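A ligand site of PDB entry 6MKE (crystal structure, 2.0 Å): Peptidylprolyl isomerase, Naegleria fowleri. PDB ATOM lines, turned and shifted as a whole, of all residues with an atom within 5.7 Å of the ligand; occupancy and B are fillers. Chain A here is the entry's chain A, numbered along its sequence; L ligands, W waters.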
ATOM      1  N   TYR A  46     -19.231 -10.068 -16.597  1.00  0.00           N
ATOM      2  CA  TYR A  46     -19.954 -11.266 -16.988  1.00  0.00           C
ATOM      3  C   TYR A  46     -19.094 -12.508 -16.789  1.00  0.00           C
ATOM      4  O   TYR A  46     -17.862 -12.446 -16.739  1.00  0.00           O
ATOM      5  CB  TYR A  46     -20.467 -11.179 -18.426  1.00  0.00           C
ATOM      6  CG  TYR A  46     -19.445 -11.426 -19.514  1.00  0.00           C
ATOM      7  CD1 TYR A  46     -19.119 -12.718 -19.916  1.00  0.00           C
ATOM      8  CD2 TYR A  46     -18.837 -10.360 -20.168  1.00  0.00           C
ATOM      9  CE1 TYR A  46     -18.189 -12.938 -20.915  1.00  0.00           C
ATOM     10  CE2 TYR A  46     -17.921 -10.571 -21.172  1.00  0.00           C
ATOM     11  CZ  TYR A  46     -17.597 -11.855 -21.547  1.00  0.00           C
ATOM     12  OH  TYR A  46     -16.674 -12.063 -22.543  1.00  0.00           O
ATOM     13  N   GLY A  48     -19.569 -16.598 -18.379  1.00  0.00           N
ATOM     14  CA  GLY A  48     -20.337 -17.512 -19.219  1.00  0.00           C
ATOM     15  C   GLY A  48     -20.008 -18.960 -18.895  1.00  0.00           C
ATOM     16  O   GLY A  48     -18.841 -19.314 -18.745  1.00  0.00           O
ATOM     17  N   PHE A  56     -16.638 -20.998 -19.776  1.00  0.00           N
ATOM     18  CA  PHE A  56     -15.930 -20.812 -21.028  1.00  0.00           C
ATOM     19  C   PHE A  56     -15.362 -19.414 -21.225  1.00  0.00           C
ATOM     20  O   PHE A  56     -14.514 -19.238 -22.111  1.00  0.00           O
ATOM     21  CB  PHE A  56     -16.817 -21.196 -22.227  1.00  0.00           C
ATOM     22  CG  PHE A  56     -18.086 -20.387 -22.355  1.00  0.00           C
ATOM     23  CD1 PHE A  56     -18.078 -19.123 -22.934  1.00  0.00           C
ATOM     24  CD2 PHE A  56     -19.311 -20.920 -21.960  1.00  0.00           C
ATOM     25  CE1 PHE A  56     -19.241 -18.392 -23.069  1.00  0.00           C
ATOM     26  CE2 PHE A  56     -20.475 -20.198 -22.092  1.00  0.00           C
ATOM     27  CZ  PHE A  56     -20.447 -18.929 -22.648  1.00  0.00           C
ATOM     28  N   ASP A  57     -15.774 -18.429 -20.431  1.00  0.00           N
ATOM     29  CA  ASP A  57     -15.223 -17.084 -20.519  1.00  0.00           C
ATOM     30  C   ASP A  57     -15.753 -16.263 -19.351  1.00  0.00           C
ATOM     31  O   ASP A  57     -16.798 -16.567 -18.776  1.00  0.00           O
ATOM     32  CB  ASP A  57     -15.581 -16.402 -21.842  1.00  0.00           C
ATOM     33  CG  ASP A  57     -14.792 -15.124 -22.070  1.00  0.00           C
ATOM     34  OD1 ASP A  57     -13.758 -14.940 -21.401  1.00  0.00           O
ATOM     35  OD2 ASP A  57     -15.208 -14.310 -22.912  1.00  0.00           O
ATOM     36  N   ARG A  62     -10.026 -10.704 -17.870  1.00  0.00           N
ATOM     37  CA  ARG A  62      -9.281  -9.592 -18.453  1.00  0.00           C
ATOM     38  C   ARG A  62      -9.233  -8.380 -17.523  1.00  0.00           C
ATOM     39  O   ARG A  62      -8.746  -7.323 -17.920  1.00  0.00           O
ATOM     40  CB  ARG A  62      -9.889  -9.211 -19.809  1.00  0.00           C
ATOM     41  CG  ARG A  62      -9.713 -10.317 -20.854  1.00  0.00           C
ATOM     42  CD  ARG A  62     -10.545 -10.093 -22.096  1.00  0.00           C
ATOM     43  NE  ARG A  62     -11.965 -10.333 -21.869  1.00  0.00           N
ATOM     44  CZ  ARG A  62     -12.512 -11.552 -21.815  1.00  0.00           C
ATOM     45  NH1 ARG A  62     -11.770 -12.636 -21.969  1.00  0.00           N
ATOM     46  NH2 ARG A  62     -13.815 -11.678 -21.610  1.00  0.00           N
ATOM     47  N   PHE A  66     -16.640  -5.361 -19.434  1.00  0.00           N
ATOM     48  CA  PHE A  66     -16.917  -5.528 -20.858  1.00  0.00           C
ATOM     49  C   PHE A  66     -17.864  -4.424 -21.313  1.00  0.00           C
ATOM     50  O   PHE A  66     -18.838  -4.100 -20.624  1.00  0.00           O
ATOM     51  CB  PHE A  66     -17.516  -6.898 -21.141  1.00  0.00           C
ATOM     52  CG  PHE A  66     -17.985  -7.076 -22.555  1.00  0.00           C
ATOM     53  CD1 PHE A  66     -17.075  -7.249 -23.576  1.00  0.00           C
ATOM     54  CD2 PHE A  66     -19.331  -7.097 -22.852  1.00  0.00           C
ATOM     55  CE1 PHE A  66     -17.509  -7.421 -24.886  1.00  0.00           C
ATOM     56  CE2 PHE A  66     -19.773  -7.256 -24.158  1.00  0.00           C
ATOM     57  CZ  PHE A  66     -18.856  -7.428 -25.172  1.00  0.00           C
ATOM     58  N   PHE A  68     -20.117  -2.790 -24.629  1.00  0.00           N
ATOM     59  CA  PHE A  68     -20.724  -2.985 -25.932  1.00  0.00           C
ATOM     60  C   PHE A  68     -21.875  -1.999 -26.084  1.00  0.00           C
ATOM     61  O   PHE A  68     -22.365  -1.438 -25.106  1.00  0.00           O
ATOM     62  CB  PHE A  68     -21.203  -4.433 -26.140  1.00  0.00           C
ATOM     63  CG  PHE A  68     -22.505  -4.760 -25.454  1.00  0.00           C
ATOM     64  CD1 PHE A  68     -23.711  -4.717 -26.147  1.00  0.00           C
ATOM     65  CD2 PHE A  68     -22.527  -5.147 -24.123  1.00  0.00           C
ATOM     66  CE1 PHE A  68     -24.908  -5.035 -25.529  1.00  0.00           C
ATOM     67  CE2 PHE A  68     -23.732  -5.473 -23.496  1.00  0.00           C
ATOM     68  CZ  PHE A  68     -24.916  -5.412 -24.199  1.00  0.00           C
ATOM     69  N   GLU A  74     -24.384  -6.117 -32.241  1.00  0.00           N
ATOM     70  CA  GLU A  74     -23.006  -6.584 -32.250  1.00  0.00           C
ATOM     71  C   GLU A  74     -22.763  -7.715 -31.261  1.00  0.00           C
ATOM     72  O   GLU A  74     -21.678  -8.305 -31.267  1.00  0.00           O
ATOM     73  CB  GLU A  74     -22.056  -5.420 -31.957  1.00  0.00           C
ATOM     74  CG  GLU A  74     -22.263  -4.767 -30.600  1.00  0.00           C
ATOM     75  CD  GLU A  74     -21.422  -3.506 -30.422  1.00  0.00           C
ATOM     76  OE1 GLU A  74     -21.160  -2.813 -31.429  1.00  0.00           O
ATOM     77  OE2 GLU A  74     -21.030  -3.209 -29.267  1.00  0.00           O
ATOM     78  N   VAL A  75     -23.738  -8.029 -30.406  1.00  0.00           N
ATOM     79  CA  VAL A  75     -23.672  -9.167 -29.504  1.00  0.00           C
ATOM     80  C   VAL A  75     -24.823 -10.102 -29.823  1.00  0.00           C
ATOM     81  O   VAL A  75     -25.727  -9.769 -30.594  1.00  0.00           O
ATOM     82  CB  VAL A  75     -23.687  -8.745 -28.018  1.00  0.00           C
ATOM     83  CG1 VAL A  75     -22.442  -7.959 -27.665  1.00  0.00           C
ATOM     84  CG2 VAL A  75     -24.935  -7.935 -27.718  1.00  0.00           C
ATOM     85  N   ILE A  76     -24.783 -11.286 -29.211  1.00  0.00           N
ATOM     86  CA  ILE A  76     -25.819 -12.282 -29.469  1.00  0.00           C
ATOM     87  C   ILE A  76     -27.175 -11.749 -29.021  1.00  0.00           C
ATOM     88  O   ILE A  76     -27.288 -10.927 -28.100  1.00  0.00           O
ATOM     89  CB  ILE A  76     -25.504 -13.624 -28.792  1.00  0.00           C
ATOM     90  CG1 ILE A  76     -25.384 -13.447 -27.273  1.00  0.00           C
ATOM     91  CG2 ILE A  76     -24.223 -14.231 -29.373  1.00  0.00           C
ATOM     92  CD1 ILE A  76     -25.057 -14.745 -26.549  1.00  0.00           C
ATOM     93  N   TRP A  79     -28.222 -11.386 -25.431  1.00  0.00           N
ATOM     94  CA  TRP A  79     -27.603 -10.306 -24.648  1.00  0.00           C
ATOM     95  C   TRP A  79     -28.296  -8.976 -24.880  1.00  0.00           C
ATOM     96  O   TRP A  79     -28.540  -8.221 -23.921  1.00  0.00           O
ATOM     97  CB  TRP A  79     -26.120 -10.201 -24.980  1.00  0.00           C
ATOM     98  CG  TRP A  79     -25.224 -10.877 -23.985  1.00  0.00           C
ATOM     99  CD1 TRP A  79     -25.197 -12.205 -23.680  1.00  0.00           C
ATOM    100  CD2 TRP A  79     -24.217 -10.261 -23.178  1.00  0.00           C
ATOM    101  NE1 TRP A  79     -24.236 -12.458 -22.720  1.00  0.00           N
ATOM    102  CE2 TRP A  79     -23.620 -11.277 -22.406  1.00  0.00           C
ATOM    103  CE3 TRP A  79     -23.748  -8.945 -23.037  1.00  0.00           C
ATOM    104  CZ2 TRP A  79     -22.584 -11.018 -21.500  1.00  0.00           C
ATOM    105  CZ3 TRP A  79     -22.733  -8.697 -22.136  1.00  0.00           C
ATOM    106  CH2 TRP A  79     -22.164  -9.726 -21.378  1.00  0.00           C
ATOM    107  N   ALA A 101     -28.395 -17.314 -29.224  1.00  0.00           N
ATOM    108  CA  ALA A 101     -26.950 -17.196 -29.093  1.00  0.00           C
ATOM    109  C   ALA A 101     -26.270 -17.477 -30.426  1.00  0.00           C
ATOM    110  O   ALA A 101     -26.465 -16.745 -31.390  1.00  0.00           O
ATOM    111  CB  ALA A 101     -26.442 -18.144 -28.001  1.00  0.00           C
ATOM    112  N   TYR A 102     -25.472 -18.547 -30.484  1.00  0.00           N
ATOM    113  CA  TYR A 102     -24.726 -18.888 -31.686  1.00  0.00           C
ATOM    114  C   TYR A 102     -25.404 -19.960 -32.526  1.00  0.00           C
ATOM    115  O   TYR A 102     -24.844 -20.370 -33.547  1.00  0.00           O
ATOM    116  CB  TYR A 102     -23.308 -19.317 -31.319  1.00  0.00           C
ATOM    117  CG  TYR A 102     -22.558 -18.231 -30.572  1.00  0.00           C
ATOM    118  CD1 TYR A 102     -22.437 -18.268 -29.193  1.00  0.00           C
ATOM    119  CD2 TYR A 102     -21.998 -17.161 -31.254  1.00  0.00           C
ATOM    120  CE1 TYR A 102     -21.776 -17.269 -28.510  1.00  0.00           C
ATOM    121  CE2 TYR A 102     -21.329 -16.154 -30.579  1.00  0.00           C
ATOM    122  CZ  TYR A 102     -21.215 -16.212 -29.202  1.00  0.00           C
ATOM    123  OH  TYR A 102     -20.546 -15.224 -28.523  1.00  0.00           O
ATOM    124  N   GLY A 103     -26.579 -20.431 -32.122  1.00  0.00           N
ATOM    125  CA  GLY A 103     -27.360 -21.334 -32.966  1.00  0.00           C
ATOM    126  C   GLY A 103     -26.622 -22.618 -33.286  1.00  0.00           C
ATOM    127  O   GLY A 103     -25.999 -23.249 -32.427  1.00  0.00           O
ATOM    128  N   ASN A 105     -23.995 -22.811 -34.992  1.00  0.00           N
ATOM    129  CA  ASN A 105     -22.564 -22.559 -35.097  1.00  0.00           C
ATOM    130  C   ASN A 105     -21.866 -22.952 -33.804  1.00  0.00           C
ATOM    131  O   ASN A 105     -22.443 -22.899 -32.724  1.00  0.00           O
ATOM    132  CB  ASN A 105     -22.291 -21.087 -35.403  1.00  0.00           C
ATOM    133  CG  ASN A 105     -22.968 -20.619 -36.678  1.00  0.00           C
ATOM    134  OD1 ASN A 105     -22.513 -20.922 -37.780  1.00  0.00           O
ATOM    135  ND2 ASN A 105     -24.056 -19.872 -36.517  1.00  0.00           N
ATOM    136  N   ILE A 107     -18.196 -22.372 -31.465  1.00  0.00           N
ATOM    137  CA  ILE A 107     -16.993 -21.596 -31.193  1.00  0.00           C
ATOM    138  C   ILE A 107     -15.865 -22.594 -30.937  1.00  0.00           C
ATOM    139  O   ILE A 107     -15.974 -23.404 -29.997  1.00  0.00           O
ATOM    140  CB  ILE A 107     -17.177 -20.655 -29.994  1.00  0.00           C
ATOM    141  CG1 ILE A 107     -18.433 -19.800 -30.185  1.00  0.00           C
ATOM    142  CG2 ILE A 107     -15.951 -19.772 -29.823  1.00  0.00           C
ATOM    143  CD1 ILE A 107     -18.417 -18.972 -31.453  1.00  0.00           C
ATOM    144  N   LEU A 110     -14.514 -24.139 -27.413  1.00  0.00           N
ATOM    145  CA  LEU A 110     -15.209 -23.558 -26.273  1.00  0.00           C
ATOM    146  C   LEU A 110     -16.680 -23.956 -26.220  1.00  0.00           C
ATOM    147  O   LEU A 110     -17.147 -24.462 -25.200  1.00  0.00           O
ATOM    148  CB  LEU A 110     -15.093 -22.033 -26.290  1.00  0.00           C
ATOM    149  CG  LEU A 110     -13.760 -21.440 -25.833  1.00  0.00           C
ATOM    150  CD1 LEU A 110     -13.877 -19.937 -25.693  1.00  0.00           C
ATOM    151  CD2 LEU A 110     -13.308 -22.077 -24.522  1.00  0.00           C
ATOM    152  N   ILE A 111     -17.412 -23.703 -27.301  1.00  0.00           N
ATOM    153  CA  ILE A 111     -18.869 -23.855 -27.292  1.00  0.00           C
ATOM    154  C   ILE A 111     -19.294 -24.775 -28.419  1.00  0.00           C
ATOM    155  O   ILE A 111     -19.157 -24.415 -29.602  1.00  0.00           O
ATOM    156  CB  ILE A 111     -19.557 -22.491 -27.401  1.00  0.00           C
ATOM    157  CG1 ILE A 111     -19.181 -21.603 -26.209  1.00  0.00           C
ATOM    158  CG2 ILE A 111     -21.065 -22.674 -27.475  1.00  0.00           C
ATOM    159  CD1 ILE A 111     -19.824 -20.233 -26.250  1.00  0.00           C
ATOM    160  N   LEU A 117     -26.491 -21.261 -23.423  1.00  0.00           N
ATOM    161  CA  LEU A 117     -25.462 -20.530 -22.690  1.00  0.00           C
ATOM    162  C   LEU A 117     -26.053 -19.940 -21.426  1.00  0.00           C
ATOM    163  O   LEU A 117     -27.158 -19.394 -21.433  1.00  0.00           O
ATOM    164  CB  LEU A 117     -24.857 -19.418 -23.556  1.00  0.00           C
ATOM    165  CG  LEU A 117     -24.203 -19.858 -24.870  1.00  0.00           C
ATOM    166  CD1 LEU A 117     -23.534 -18.667 -25.553  1.00  0.00           C
ATOM    167  CD2 LEU A 117     -23.203 -20.977 -24.620  1.00  0.00           C
ATOM    168  N   PHE A 119     -25.261 -17.109 -18.542  1.00  0.00           N
ATOM    169  CA  PHE A 119     -24.467 -15.908 -18.323  1.00  0.00           C
ATOM    170  C   PHE A 119     -24.862 -15.238 -17.007  1.00  0.00           C
ATOM    171  O   PHE A 119     -26.044 -15.012 -16.749  1.00  0.00           O
ATOM    172  CB  PHE A 119     -24.636 -14.891 -19.458  1.00  0.00           C
ATOM    173  CG  PHE A 119     -23.811 -15.186 -20.673  1.00  0.00           C
ATOM    174  CD1 PHE A 119     -22.463 -14.881 -20.703  1.00  0.00           C
ATOM    175  CD2 PHE A 119     -24.394 -15.749 -21.800  1.00  0.00           C
ATOM    176  CE1 PHE A 119     -21.708 -15.138 -21.824  1.00  0.00           C
ATOM    177  CE2 PHE A 119     -23.639 -16.006 -22.921  1.00  0.00           C
ATOM    178  CZ  PHE A 119     -22.293 -15.696 -22.937  1.00  0.00           C
HETATM  179  C1  LIG L   1     -21.088 -11.969 -27.746  1.00  0.00           C
HETATM  180  C2  LIG L   1     -21.197 -12.594 -26.350  1.00  0.00           C
HETATM  181  C3  LIG L   1     -21.944 -11.683 -25.377  1.00  0.00           C
HETATM  182  C4  LIG L   1     -21.051 -10.551 -24.903  1.00  0.00           C
HETATM  183  C5  LIG L   1     -19.767 -11.078 -24.300  1.00  0.00           C
HETATM  184  C6  LIG L   1     -19.032 -11.959 -25.282  1.00  0.00           C
HETATM  185  C7  LIG L   1     -19.683 -14.331 -25.634  1.00  0.00           C
HETATM  186  C8  LIG L   1     -18.423 -14.802 -24.902  1.00  0.00           C
HETATM  187  C9  LIG L   1     -17.149 -15.150 -25.715  1.00  0.00           C
HETATM  188  C10 LIG L   1     -17.486 -15.595 -27.141  1.00  0.00           C
HETATM  189  C11 LIG L   1     -16.240 -15.487 -28.036  1.00  0.00           C
HETATM  190  C12 LIG L   1     -15.583 -14.127 -27.937  1.00  0.00           C
HETATM  191  C13 LIG L   1     -15.287 -13.805 -26.473  1.00  0.00           C
HETATM  192  C14 LIG L   1     -14.705 -12.424 -26.231  1.00  0.00           C
HETATM  193  C15 LIG L   1     -15.426 -11.292 -26.933  1.00  0.00           C
HETATM  194  C16 LIG L   1     -15.023  -9.880 -26.485  1.00  0.00           C
HETATM  195  C17 LIG L   1     -13.778  -9.390 -27.228  1.00  0.00           C
HETATM  196  C18 LIG L   1     -13.995  -8.972 -28.666  1.00  0.00           C
HETATM  197  C19 LIG L   1     -13.941  -9.852 -29.657  1.00  0.00           C
HETATM  198  C20 LIG L   1     -14.245  -9.611 -31.113  1.00  0.00           C
HETATM  199  C21 LIG L   1     -15.679 -10.092 -31.358  1.00  0.00           C
HETATM  200  C22 LIG L   1     -16.761  -9.110 -30.975  1.00  0.00           C
HETATM  201  C23 LIG L   1     -18.160  -9.707 -30.803  1.00  0.00           C
HETATM  202  C24 LIG L   1     -18.378 -10.449 -29.471  1.00  0.00           C
HETATM  203  C25 LIG L   1     -19.693 -11.249 -29.502  1.00  0.00           C
HETATM  204  C26 LIG L   1     -19.774 -12.280 -30.609  1.00  0.00           C
HETATM  205  C27 LIG L   1     -20.680 -12.174 -31.569  1.00  0.00           C
HETATM  206  C28 LIG L   1     -20.848 -13.026 -32.790  1.00  0.00           C
HETATM  207  C29 LIG L   1     -22.330 -13.348 -33.031  1.00  0.00           C
HETATM  208  C30 LIG L   1     -22.561 -14.200 -34.264  1.00  0.00           C
HETATM  209  C31 LIG L   1     -22.005 -13.458 -35.474  1.00  0.00           C
HETATM  210  C32 LIG L   1     -20.533 -13.151 -35.289  1.00  0.00           C
HETATM  211  C33 LIG L   1     -20.290 -12.324 -34.033  1.00  0.00           C
HETATM  212  C34 LIG L   1     -18.055 -17.009 -27.197  1.00  0.00           C
HETATM  213  C35 LIG L   1     -14.777  -9.835 -24.979  1.00  0.00           C
HETATM  214  C36 LIG L   1     -14.349  -7.519 -28.862  1.00  0.00           C
HETATM  215  C37 LIG L   1     -13.241 -10.383 -31.994  1.00  0.00           C
HETATM  216  C38 LIG L   1     -13.323  -9.991 -33.437  1.00  0.00           C
HETATM  217  C39 LIG L   1     -12.882  -8.892 -33.952  1.00  0.00           C
HETATM  218  C40 LIG L   1     -18.341  -9.487 -28.283  1.00  0.00           C
HETATM  219  C41 LIG L   1     -18.766 -13.397 -30.543  1.00  0.00           C
HETATM  220  C42 LIG L   1     -14.583 -14.009 -30.096  1.00  0.00           C
HETATM  221  C43 LIG L   1     -12.429 -12.624 -25.551  1.00  0.00           C
HETATM  222  C44 LIG L   1     -24.392 -15.718 -34.184  1.00  0.00           C
HETATM  223  N1  LIG L   1     -19.916 -13.022 -25.767  1.00  0.00           N
HETATM  224  O1  LIG L   1     -19.829 -11.869 -28.205  1.00  0.00           O
HETATM  225  O2  LIG L   1     -22.040 -11.602 -28.361  1.00  0.00           O
HETATM  226  O3  LIG L   1     -20.443 -15.202 -26.044  1.00  0.00           O
HETATM  227  O4  LIG L   1     -18.438 -14.889 -23.688  1.00  0.00           O
HETATM  228  O5  LIG L   1     -16.498 -13.890 -25.721  1.00  0.00           O
HETATM  229  O6  LIG L   1     -16.249 -16.058 -25.155  1.00  0.00           O
HETATM  230  O7  LIG L   1     -14.379 -14.115 -28.692  1.00  0.00           O
HETATM  231  O8  LIG L   1     -13.339 -12.457 -26.630  1.00  0.00           O
HETATM  232  O9  LIG L   1     -15.941 -11.180 -31.817  1.00  0.00           O
HETATM  233  O10 LIG L   1     -19.123  -8.663 -30.905  1.00  0.00           O
HETATM  234  O11 LIG L   1     -23.943 -14.410 -34.498  1.00  0.00           O
HETATM  235  O12 LIG L   1     -22.217 -14.217 -36.665  1.00  0.00           O
HETATM  236  O   HOH W   1     -14.409  -6.115 -25.699  1.00  0.00           O
HETATM  237  O   HOH W   2     -26.647 -13.074 -33.903  1.00  0.00           O
HETATM  238  O   HOH W   3     -11.999 -12.340 -28.939  1.00  0.00           O
HETATM  239  O   HOH W   4     -25.000 -14.460 -37.903  1.00  0.00           O
HETATM  240  O   HOH W   5     -18.856  -5.939 -29.605  1.00  0.00           O
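The backbone carbonyl oxygen (O) of Tyr 102 sits at hydrogen-bond distance from the side-chain amide nitrogen (ND2) of Asn 105 (3.1 Å). The side-chain carboxylate (OD2) of Asp 57 sits at hydrogen-bond distance from the side-chain hydroxyl (OH) of Tyr 46 (2.7 Å). The guanidinium group (NH1) of Arg 62 is in salt-bridge range of the side-chain carboxylate (OD1) of Asp 57. The backbone carbonyl oxygen (O) of Asp 57 is in hydrogen-bond range of the backbone NH (N) of Gly 48 (2.8 Å). The guanidinium group (NH2) of Arg 62 sits at hydrogen-bond distance from the side-chain hydroxyl (OH) of Tyr 46, at 3.0 Å. The backbone NH of Phe 56 is in hydrogen-bond range of the backbone carbonyl oxygen of Gly 48, 3.0 Å away.
The side-chain hydroxyl (OH) of Tyr 102 sits at hydrogen-bond distance from an oxygen (O3) of the ligand, 2.5 Å away. The backbone carbonyl oxygen of Glu 74 sits at hydrogen-bond distance from an oxygen (O10) of the ligand (2.6 Å). O2 of the ligand is in hydrogen-bond range of N of Ile 76, at 2.9 Å. O6 of the ligand sits at hydrogen-bond distance from OD2 of Asp 57, at 3.0 Å.
Tyr 46 touches the ligand (CE1 to O4, 3.4 Å). CE1 of Phe 56 touches O4 of the ligand, at 3.6 Å. Arg 62 touches the ligand. Phe 66 touches the ligand. CA of Val 75 touches O2 of the ligand, at 3.1 Å. Trp 79 touches the ligand. Ala 101 touches the ligand. Ile 111 touches the ligand. Phe 119 touches the ligand (CZ to O3, 3.6 Å).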
